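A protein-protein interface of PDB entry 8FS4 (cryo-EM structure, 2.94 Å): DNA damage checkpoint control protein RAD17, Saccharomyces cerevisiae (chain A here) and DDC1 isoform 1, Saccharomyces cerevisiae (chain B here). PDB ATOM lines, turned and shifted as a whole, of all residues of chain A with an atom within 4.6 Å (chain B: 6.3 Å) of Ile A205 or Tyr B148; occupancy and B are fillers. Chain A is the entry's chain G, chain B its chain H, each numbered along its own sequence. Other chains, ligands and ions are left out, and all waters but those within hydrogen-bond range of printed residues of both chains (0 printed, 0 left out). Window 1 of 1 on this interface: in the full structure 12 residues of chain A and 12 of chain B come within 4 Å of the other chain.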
ATOM      1  N   ALA A 166     -11.983  14.905  20.630  1.00  0.00           N
ATOM      2  CA  ALA A 166     -11.089  15.757  21.409  1.00  0.00           C
ATOM      3  C   ALA A 166     -10.425  16.807  20.527  1.00  0.00           C
ATOM      4  O   ALA A 166     -10.314  17.975  20.915  1.00  0.00           O
ATOM      5  CB  ALA A 166     -10.035  14.904  22.112  1.00  0.00           C
ATOM      6  N   ASP A 169     -12.939  19.461  19.630  1.00  0.00           N
ATOM      7  CA  ASP A 169     -13.142  20.350  20.770  1.00  0.00           C
ATOM      8  C   ASP A 169     -11.985  21.330  20.910  1.00  0.00           C
ATOM      9  O   ASP A 169     -12.199  22.528  21.129  1.00  0.00           O
ATOM     10  CB  ASP A 169     -13.308  19.530  22.049  1.00  0.00           C
ATOM     11  CG  ASP A 169     -14.755  19.431  22.493  1.00  0.00           C
ATOM     12  OD1 ASP A 169     -15.349  20.478  22.826  1.00  0.00           O
ATOM     13  OD2 ASP A 169     -15.298  18.305  22.511  1.00  0.00           O
ATOM     14  N   LEU A 170     -10.751  20.843  20.776  1.00  0.00           N
ATOM     15  CA  LEU A 170      -9.594  21.725  20.886  1.00  0.00           C
ATOM     16  C   LEU A 170      -9.605  22.778  19.786  1.00  0.00           C
ATOM     17  O   LEU A 170      -9.230  23.933  20.016  1.00  0.00           O
ATOM     18  CB  LEU A 170      -8.305  20.903  20.842  1.00  0.00           C
ATOM     19  CG  LEU A 170      -7.861  20.183  22.125  1.00  0.00           C
ATOM     20  CD1 LEU A 170      -6.353  19.997  22.139  1.00  0.00           C
ATOM     21  CD2 LEU A 170      -8.299  20.908  23.392  1.00  0.00           C
ATOM     22  N   ILE A 173     -12.075  25.390  20.842  1.00  0.00           N
ATOM     23  CA  ILE A 173     -11.545  26.229  21.914  1.00  0.00           C
ATOM     24  C   ILE A 173     -10.409  27.120  21.434  1.00  0.00           C
ATOM     25  O   ILE A 173      -9.933  27.969  22.197  1.00  0.00           O
ATOM     26  CB  ILE A 173     -11.071  25.357  23.094  1.00  0.00           C
ATOM     27  CG1 ILE A 173     -12.154  24.358  23.514  1.00  0.00           C
ATOM     28  CG2 ILE A 173     -10.738  26.205  24.305  1.00  0.00           C
ATOM     29  CD1 ILE A 173     -11.598  23.079  24.099  1.00  0.00           C
ATOM     30  N   PHE A 192      -4.279   9.827  30.583  1.00  0.00           N
ATOM     31  CA  PHE A 192      -3.889  10.403  29.301  1.00  0.00           C
ATOM     32  C   PHE A 192      -4.768  11.617  29.051  1.00  0.00           C
ATOM     33  O   PHE A 192      -5.995  11.492  28.995  1.00  0.00           O
ATOM     34  CB  PHE A 192      -4.036   9.382  28.169  1.00  0.00           C
ATOM     35  CG  PHE A 192      -3.492   9.854  26.852  1.00  0.00           C
ATOM     36  CD1 PHE A 192      -2.150   9.706  26.546  1.00  0.00           C
ATOM     37  CD2 PHE A 192      -4.324  10.436  25.915  1.00  0.00           C
ATOM     38  CE1 PHE A 192      -1.652  10.139  25.335  1.00  0.00           C
ATOM     39  CE2 PHE A 192      -3.833  10.868  24.704  1.00  0.00           C
ATOM     40  CZ  PHE A 192      -2.496  10.719  24.413  1.00  0.00           C
ATOM     41  N   ALA A 193      -4.147  12.785  28.902  1.00  0.00           N
ATOM     42  CA  ALA A 193      -4.882  14.034  28.778  1.00  0.00           C
ATOM     43  C   ALA A 193      -4.274  14.882  27.672  1.00  0.00           C
ATOM     44  O   ALA A 193      -3.095  14.750  27.332  1.00  0.00           O
ATOM     45  CB  ALA A 193      -4.888  14.817  30.097  1.00  0.00           C
ATOM     46  N   LEU A 194      -5.103  15.759  27.113  1.00  0.00           N
ATOM     47  CA  LEU A 194      -4.708  16.697  26.063  1.00  0.00           C
ATOM     48  C   LEU A 194      -5.019  18.100  26.576  1.00  0.00           C
ATOM     49  O   LEU A 194      -6.135  18.599  26.416  1.00  0.00           O
ATOM     50  CB  LEU A 194      -5.438  16.401  24.750  1.00  0.00           C
ATOM     51  CG  LEU A 194      -5.008  15.144  23.991  1.00  0.00           C
ATOM     52  CD1 LEU A 194      -5.958  14.875  22.836  1.00  0.00           C
ATOM     53  CD2 LEU A 194      -3.579  15.271  23.489  1.00  0.00           C
ATOM     54  N   LEU A 200      -9.808  30.418  26.561  1.00  0.00           N
ATOM     55  CA  LEU A 200     -10.486  30.083  27.809  1.00  0.00           C
ATOM     56  C   LEU A 200      -9.503  30.001  28.968  1.00  0.00           C
ATOM     57  O   LEU A 200      -9.898  30.150  30.130  1.00  0.00           O
ATOM     58  CB  LEU A 200     -11.236  28.759  27.657  1.00  0.00           C
ATOM     59  CG  LEU A 200     -12.670  28.841  27.129  1.00  0.00           C
ATOM     60  CD1 LEU A 200     -12.712  29.549  25.786  1.00  0.00           C
ATOM     61  CD2 LEU A 200     -13.278  27.455  27.019  1.00  0.00           C
ATOM     62  N   PHE A 202      -6.556  27.585  30.688  1.00  0.00           N
ATOM     63  CA  PHE A 202      -5.890  26.289  30.774  1.00  0.00           C
ATOM     64  C   PHE A 202      -6.975  25.215  30.778  1.00  0.00           C
ATOM     65  O   PHE A 202      -7.541  24.894  31.828  1.00  0.00           O
ATOM     66  CB  PHE A 202      -5.008  26.211  32.017  1.00  0.00           C
ATOM     67  CG  PHE A 202      -3.607  25.748  31.738  1.00  0.00           C
ATOM     68  CD1 PHE A 202      -2.727  26.537  31.021  1.00  0.00           C
ATOM     69  CD2 PHE A 202      -3.173  24.522  32.195  1.00  0.00           C
ATOM     70  CE1 PHE A 202      -1.440  26.102  30.768  1.00  0.00           C
ATOM     71  CE2 PHE A 202      -1.895  24.082  31.947  1.00  0.00           C
ATOM     72  CZ  PHE A 202      -1.025  24.872  31.233  1.00  0.00           C
ATOM     73  N   SER A 203      -7.264  24.668  29.601  1.00  0.00           N
ATOM     74  CA  SER A 203      -8.300  23.660  29.431  1.00  0.00           C
ATOM     75  C   SER A 203      -7.665  22.283  29.315  1.00  0.00           C
ATOM     76  O   SER A 203      -6.565  22.138  28.773  1.00  0.00           O
ATOM     77  CB  SER A 203      -9.147  23.954  28.193  1.00  0.00           C
ATOM     78  OG  SER A 203      -9.726  22.767  27.678  1.00  0.00           O
ATOM     79  N   LYS A 204      -8.361  21.274  29.833  1.00  0.00           N
ATOM     80  CA  LYS A 204      -7.869  19.906  29.844  1.00  0.00           C
ATOM     81  C   LYS A 204      -8.936  18.972  29.294  1.00  0.00           C
ATOM     82  O   LYS A 204     -10.115  19.083  29.644  1.00  0.00           O
ATOM     83  CB  LYS A 204      -7.478  19.477  31.266  1.00  0.00           C
ATOM     84  CG  LYS A 204      -6.943  18.051  31.385  1.00  0.00           C
ATOM     85  CD  LYS A 204      -7.217  17.421  32.754  1.00  0.00           C
ATOM     86  CE  LYS A 204      -6.909  18.346  33.932  1.00  0.00           C
ATOM     87  NZ  LYS A 204      -7.722  17.987  35.124  1.00  0.00           N
ATOM     88  N   ILE A 205      -8.511  18.055  28.430  1.00  0.00           N
ATOM     89  CA  ILE A 205      -9.349  16.968  27.938  1.00  0.00           C
ATOM     90  C   ILE A 205      -8.672  15.678  28.378  1.00  0.00           C
ATOM     91  O   ILE A 205      -7.580  15.348  27.900  1.00  0.00           O
ATOM     92  CB  ILE A 205      -9.528  17.004  26.413  1.00  0.00           C
ATOM     93  CG1 ILE A 205      -9.622  18.447  25.896  1.00  0.00           C
ATOM     94  CG2 ILE A 205     -10.755  16.193  26.006  1.00  0.00           C
ATOM     95  CD1 ILE A 205     -10.928  19.149  26.220  1.00  0.00           C
ATOM     96  N   LYS A 206      -9.313  14.950  29.287  1.00  0.00           N
ATOM     97  CA  LYS A 206      -8.744  13.741  29.871  1.00  0.00           C
ATOM     98  C   LYS A 206      -9.390  12.524  29.225  1.00  0.00           C
ATOM     99  O   LYS A 206     -10.616  12.376  29.259  1.00  0.00           O
ATOM    100  CB  LYS A 206      -8.961  13.718  31.383  1.00  0.00           C
ATOM    101  CG  LYS A 206      -8.228  12.601  32.110  1.00  0.00           C
ATOM    102  CD  LYS A 206      -7.389  13.135  33.263  1.00  0.00           C
ATOM    103  CE  LYS A 206      -8.239  13.448  34.487  1.00  0.00           C
ATOM    104  NZ  LYS A 206      -7.527  13.123  35.755  1.00  0.00           N
ATOM    105  N   LEU A 207      -8.569  11.661  28.640  1.00  0.00           N
ATOM    106  CA  LEU A 207      -9.090  10.428  28.075  1.00  0.00           C
ATOM    107  C   LEU A 207      -9.379   9.432  29.197  1.00  0.00           C
ATOM    108  O   LEU A 207      -8.641   9.380  30.186  1.00  0.00           O
ATOM    109  CB  LEU A 207      -8.101   9.830  27.075  1.00  0.00           C
ATOM    110  CG  LEU A 207      -8.182  10.331  25.628  1.00  0.00           C
ATOM    111  CD1 LEU A 207      -9.592  10.216  25.058  1.00  0.00           C
ATOM    112  CD2 LEU A 207      -7.690  11.767  25.529  1.00  0.00           C
ATOM    113  N   THR B 103     -18.716  28.264  24.467  1.00  0.00           N
ATOM    114  CA  THR B 103     -18.110  27.087  23.860  1.00  0.00           C
ATOM    115  C   THR B 103     -17.978  25.935  24.845  1.00  0.00           C
ATOM    116  O   THR B 103     -17.981  24.770  24.430  1.00  0.00           O
ATOM    117  CB  THR B 103     -16.726  27.428  23.299  1.00  0.00           C
ATOM    118  OG1 THR B 103     -15.824  27.702  24.378  1.00  0.00           O
ATOM    119  CG2 THR B 103     -16.800  28.639  22.382  1.00  0.00           C
ATOM    120  N   ILE B 104     -17.859  26.235  26.139  1.00  0.00           N
ATOM    121  CA  ILE B 104     -17.808  25.173  27.139  1.00  0.00           C
ATOM    122  C   ILE B 104     -19.151  24.464  27.218  1.00  0.00           C
ATOM    123  O   ILE B 104     -19.217  23.230  27.296  1.00  0.00           O
ATOM    124  CB  ILE B 104     -17.391  25.730  28.513  1.00  0.00           C
ATOM    125  CG1 ILE B 104     -16.245  26.741  28.390  1.00  0.00           C
ATOM    126  CG2 ILE B 104     -16.986  24.584  29.421  1.00  0.00           C
ATOM    127  CD1 ILE B 104     -15.893  27.438  29.694  1.00  0.00           C
ATOM    128  N   LEU B 134     -13.433  30.763  37.330  1.00  0.00           N
ATOM    129  CA  LEU B 134     -14.580  29.868  37.415  1.00  0.00           C
ATOM    130  C   LEU B 134     -14.158  28.424  37.165  1.00  0.00           C
ATOM    131  O   LEU B 134     -13.170  28.153  36.475  1.00  0.00           O
ATOM    132  CB  LEU B 134     -15.636  30.302  36.394  1.00  0.00           C
ATOM    133  CG  LEU B 134     -17.065  29.758  36.454  1.00  0.00           C
ATOM    134  CD1 LEU B 134     -17.845  30.389  37.584  1.00  0.00           C
ATOM    135  CD2 LEU B 134     -17.764  30.017  35.128  1.00  0.00           C
ATOM    136  N   ILE B 135     -14.917  27.491  37.737  1.00  0.00           N
ATOM    137  CA  ILE B 135     -14.669  26.059  37.599  1.00  0.00           C
ATOM    138  C   ILE B 135     -15.904  25.430  36.972  1.00  0.00           C
ATOM    139  O   ILE B 135     -17.024  25.628  37.460  1.00  0.00           O
ATOM    140  CB  ILE B 135     -14.350  25.397  38.951  1.00  0.00           C
ATOM    141  CG1 ILE B 135     -12.965  25.812  39.467  1.00  0.00           C
ATOM    142  CG2 ILE B 135     -14.430  23.874  38.845  1.00  0.00           C
ATOM    143  CD1 ILE B 135     -11.841  25.712  38.448  1.00  0.00           C
ATOM    144  N   VAL B 136     -15.700  24.674  35.896  1.00  0.00           N
ATOM    145  CA  VAL B 136     -16.764  23.938  35.224  1.00  0.00           C
ATOM    146  C   VAL B 136     -16.228  22.563  34.852  1.00  0.00           C
ATOM    147  O   VAL B 136     -15.120  22.448  34.317  1.00  0.00           O
ATOM    148  CB  VAL B 136     -17.272  24.685  33.976  1.00  0.00           C
ATOM    149  CG1 VAL B 136     -16.228  24.650  32.884  1.00  0.00           C
ATOM    150  CG2 VAL B 136     -18.585  24.089  33.491  1.00  0.00           C
ATOM    151  N   VAL B 137     -17.010  21.524  35.137  1.00  0.00           N
ATOM    152  CA  VAL B 137     -16.613  20.139  34.910  1.00  0.00           C
ATOM    153  C   VAL B 137     -17.574  19.525  33.903  1.00  0.00           C
ATOM    154  O   VAL B 137     -18.796  19.668  34.036  1.00  0.00           O
ATOM    155  CB  VAL B 137     -16.606  19.326  36.218  1.00  0.00           C
ATOM    156  CG1 VAL B 137     -16.022  17.939  35.987  1.00  0.00           C
ATOM    157  CG2 VAL B 137     -15.847  20.065  37.312  1.00  0.00           C
ATOM    158  N   ILE B 138     -17.023  18.848  32.898  1.00  0.00           N
ATOM    159  CA  ILE B 138     -17.803  18.151  31.882  1.00  0.00           C
ATOM    160  C   ILE B 138     -17.411  16.683  31.913  1.00  0.00           C
ATOM    161  O   ILE B 138     -16.222  16.353  31.841  1.00  0.00           O
ATOM    162  CB  ILE B 138     -17.576  18.743  30.479  1.00  0.00           C
ATOM    163  CG1 ILE B 138     -17.897  20.238  30.480  1.00  0.00           C
ATOM    164  CG2 ILE B 138     -18.431  18.013  29.449  1.00  0.00           C
ATOM    165  CD1 ILE B 138     -17.576  20.941  29.180  1.00  0.00           C
ATOM    166  N   ILE B 144     -15.318  10.600  29.092  1.00  0.00           N
ATOM    167  CA  ILE B 144     -14.329  11.650  28.869  1.00  0.00           C
ATOM    168  C   ILE B 144     -14.665  12.822  29.783  1.00  0.00           C
ATOM    169  O   ILE B 144     -15.783  13.344  29.752  1.00  0.00           O
ATOM    170  CB  ILE B 144     -14.304  12.086  27.396  1.00  0.00           C
ATOM    171  CG1 ILE B 144     -13.895  10.907  26.508  1.00  0.00           C
ATOM    172  CG2 ILE B 144     -13.354  13.274  27.205  1.00  0.00           C
ATOM    173  CD1 ILE B 144     -13.650  11.260  25.052  1.00  0.00           C
ATOM    174  N   VAL B 145     -13.696  13.238  30.594  1.00  0.00           N
ATOM    175  CA  VAL B 145     -13.857  14.367  31.504  1.00  0.00           C
ATOM    176  C   VAL B 145     -13.020  15.523  30.979  1.00  0.00           C
ATOM    177  O   VAL B 145     -11.812  15.376  30.757  1.00  0.00           O
ATOM    178  CB  VAL B 145     -13.466  14.005  32.951  1.00  0.00           C
ATOM    179  CG1 VAL B 145     -12.073  13.407  33.020  1.00  0.00           C
ATOM    180  CG2 VAL B 145     -13.552  15.235  33.851  1.00  0.00           C
ATOM    181  N   LYS B 146     -13.665  16.669  30.775  1.00  0.00           N
ATOM    182  CA  LYS B 146     -13.018  17.876  30.280  1.00  0.00           C
ATOM    183  C   LYS B 146     -13.018  18.927  31.379  1.00  0.00           C
ATOM    184  O   LYS B 146     -14.049  19.162  32.018  1.00  0.00           O
ATOM    185  CB  LYS B 146     -13.736  18.412  29.040  1.00  0.00           C
ATOM    186  CG  LYS B 146     -14.008  17.365  27.973  1.00  0.00           C
ATOM    187  CD  LYS B 146     -14.474  17.990  26.663  1.00  0.00           C
ATOM    188  CE  LYS B 146     -15.666  18.913  26.862  1.00  0.00           C
ATOM    189  NZ  LYS B 146     -16.221  19.401  25.570  1.00  0.00           N
ATOM    190  N   GLU B 147     -11.868  19.559  31.592  1.00  0.00           N
ATOM    191  CA  GLU B 147     -11.698  20.566  32.630  1.00  0.00           C
ATOM    192  C   GLU B 147     -11.424  21.919  31.987  1.00  0.00           C
ATOM    193  O   GLU B 147     -10.592  22.023  31.080  1.00  0.00           O
ATOM    194  CB  GLU B 147     -10.554  20.189  33.573  1.00  0.00           C
ATOM    195  CG  GLU B 147     -11.000  19.671  34.932  1.00  0.00           C
ATOM    196  CD  GLU B 147     -11.797  20.691  35.720  1.00  0.00           C
ATOM    197  OE1 GLU B 147     -11.566  21.904  35.534  1.00  0.00           O
ATOM    198  OE2 GLU B 147     -12.652  20.279  36.529  1.00  0.00           O
ATOM    199  N   TYR B 148     -12.127  22.948  32.458  1.00  0.00           N
ATOM    200  CA  TYR B 148     -11.931  24.315  32.000  1.00  0.00           C
ATOM    201  C   TYR B 148     -11.835  25.239  33.205  1.00  0.00           C
ATOM    202  O   TYR B 148     -12.457  24.999  34.242  1.00  0.00           O
ATOM    203  CB  TYR B 148     -13.073  24.779  31.089  1.00  0.00           C
ATOM    204  CG  TYR B 148     -13.263  23.937  29.851  1.00  0.00           C
ATOM    205  CD1 TYR B 148     -13.969  22.743  29.902  1.00  0.00           C
ATOM    206  CD2 TYR B 148     -12.748  24.340  28.627  1.00  0.00           C
ATOM    207  CE1 TYR B 148     -14.147  21.971  28.773  1.00  0.00           C
ATOM    208  CE2 TYR B 148     -12.923  23.574  27.491  1.00  0.00           C
ATOM    209  CZ  TYR B 148     -13.625  22.391  27.571  1.00  0.00           C
ATOM    210  OH  TYR B 148     -13.806  21.620  26.447  1.00  0.00           O
ATOM    211  N   CYS B 149     -11.044  26.301  33.060  1.00  0.00           N
ATOM    212  CA  CYS B 149     -10.824  27.283  34.122  1.00  0.00           C
ATOM    213  C   CYS B 149     -10.970  28.689  33.552  1.00  0.00           C
ATOM    214  O   CYS B 149      -9.986  29.428  33.425  1.00  0.00           O
ATOM    215  CB  CYS B 149      -9.448  27.094  34.760  1.00  0.00           C
ATOM    216  SG  CYS B 149      -9.320  25.653  35.841  1.00  0.00           S
ATOM    217  N   PRO B 150     -12.188  29.093  33.197  1.00  0.00           N
ATOM    218  CA  PRO B 150     -12.389  30.467  32.722  1.00  0.00           C
ATOM    219  C   PRO B 150     -12.321  31.464  33.868  1.00  0.00           C
ATOM    220  O   PRO B 150     -12.849  31.227  34.957  1.00  0.00           O
ATOM    221  CB  PRO B 150     -13.784  30.425  32.088  1.00  0.00           C
ATOM    222  CG  PRO B 150     -14.479  29.311  32.773  1.00  0.00           C
ATOM    223  CD  PRO B 150     -13.430  28.301  33.152  1.00  0.00           C
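Of the printed residues of chain B, Phe A202 touches Cys B149 (3.97 Å).
Of the printed residues of chain B, Ser A203 touches Glu B147 and Tyr B148.
Ile A205 touches just these residues of chain B: Val B145 (3.95 Å), Lys B146 (3.8 Å) and Tyr B148 (3.8 Å).
Tyr B148 touches just these residues of chain A: Ile A173 (3.5 Å), Leu A200 (3.5 Å), Ser A203 (3.3 Å) and Ile A205 (3.8 Å).
Of the printed residues of chain A, Cys B149 touches Leu A200 (3.4 Å) and Phe A202 (3.97 Å).
Of the printed residues of chain A, Pro B150 touches Leu A200.
The nearest residue of chain B that does not touch Ile A205 is Ile B144 (4.1 Å).
The nearest printed residue of chain B that does not touch Lys A206 is Lys B146 (4.8 Å).
The backbone NH of Leu A194 lies within hydrogen-bond range of the backbone carbonyl oxygen of Ile A205.
O of Pro B150 lies within hydrogen-bond range of N of Leu B134.
The backbone carbonyl oxygen (O) of Ile B138 sits at hydrogen-bond distance from the backbone NH (N) of Lys B146, at 2.8 Å.
The side-chain hydroxyl of Tyr B148 lies close to the side-chain amino group of Lys B146, at 3.4 Å.
The side-chain amino group (NZ) of Lys B146 lies within salt-bridge range of the side-chain carboxylate (OD1) of Asp A169 (3.1 Å).
O of Glu B147 lies within hydrogen-bond range of N of Lys A204 (2.7 Å).
O of Val B145 sits at hydrogen-bond distance from N of Lys A206 (2.9 Å).
O of Leu A200 lies close to O of Cys B149, 3.4 Å away.
Hydrophobic or aromatic side chains of chain A within 4 Å of the printed part of chain B: Ile A173, Leu A200 and Ile A205.
Hydrophobic or aromatic side chains of chain B that line the printed part of chain A: Ile B104, Ile B144, Val B145 and Tyr B148.
Among the printed residues, Asp or Glu carboxylates within 4 Å of a Lys or Arg side-chain nitrogen of the other chain: Asp A169 with Lys B146.
Thr B103 touches Leu A200.
Leu A200 touches Ile B104 (CD2 to CG1, 3.3 Å).
CD2 of Leu A200 touches CD2 of Tyr B148, 3.5 Å away.
Pro B150 touches Leu A200 (CA to O, 3.6 Å).
Cys B149 touches Phe A202 (N to O, 3.97 Å).
CA of Ser A203 touches O of Glu B147, at 3.3 Å.
O of Lys A204 touches CA of Lys B146, 3.2 Å away.
Ile A205 touches Val B145 (C to O, 3.95 Å).
Ile A205 touches Lys B146 (CD1 to CD, 3.8 Å).
CG2 of Ile B144 touches O of Lys A206, at 3.5 Å.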
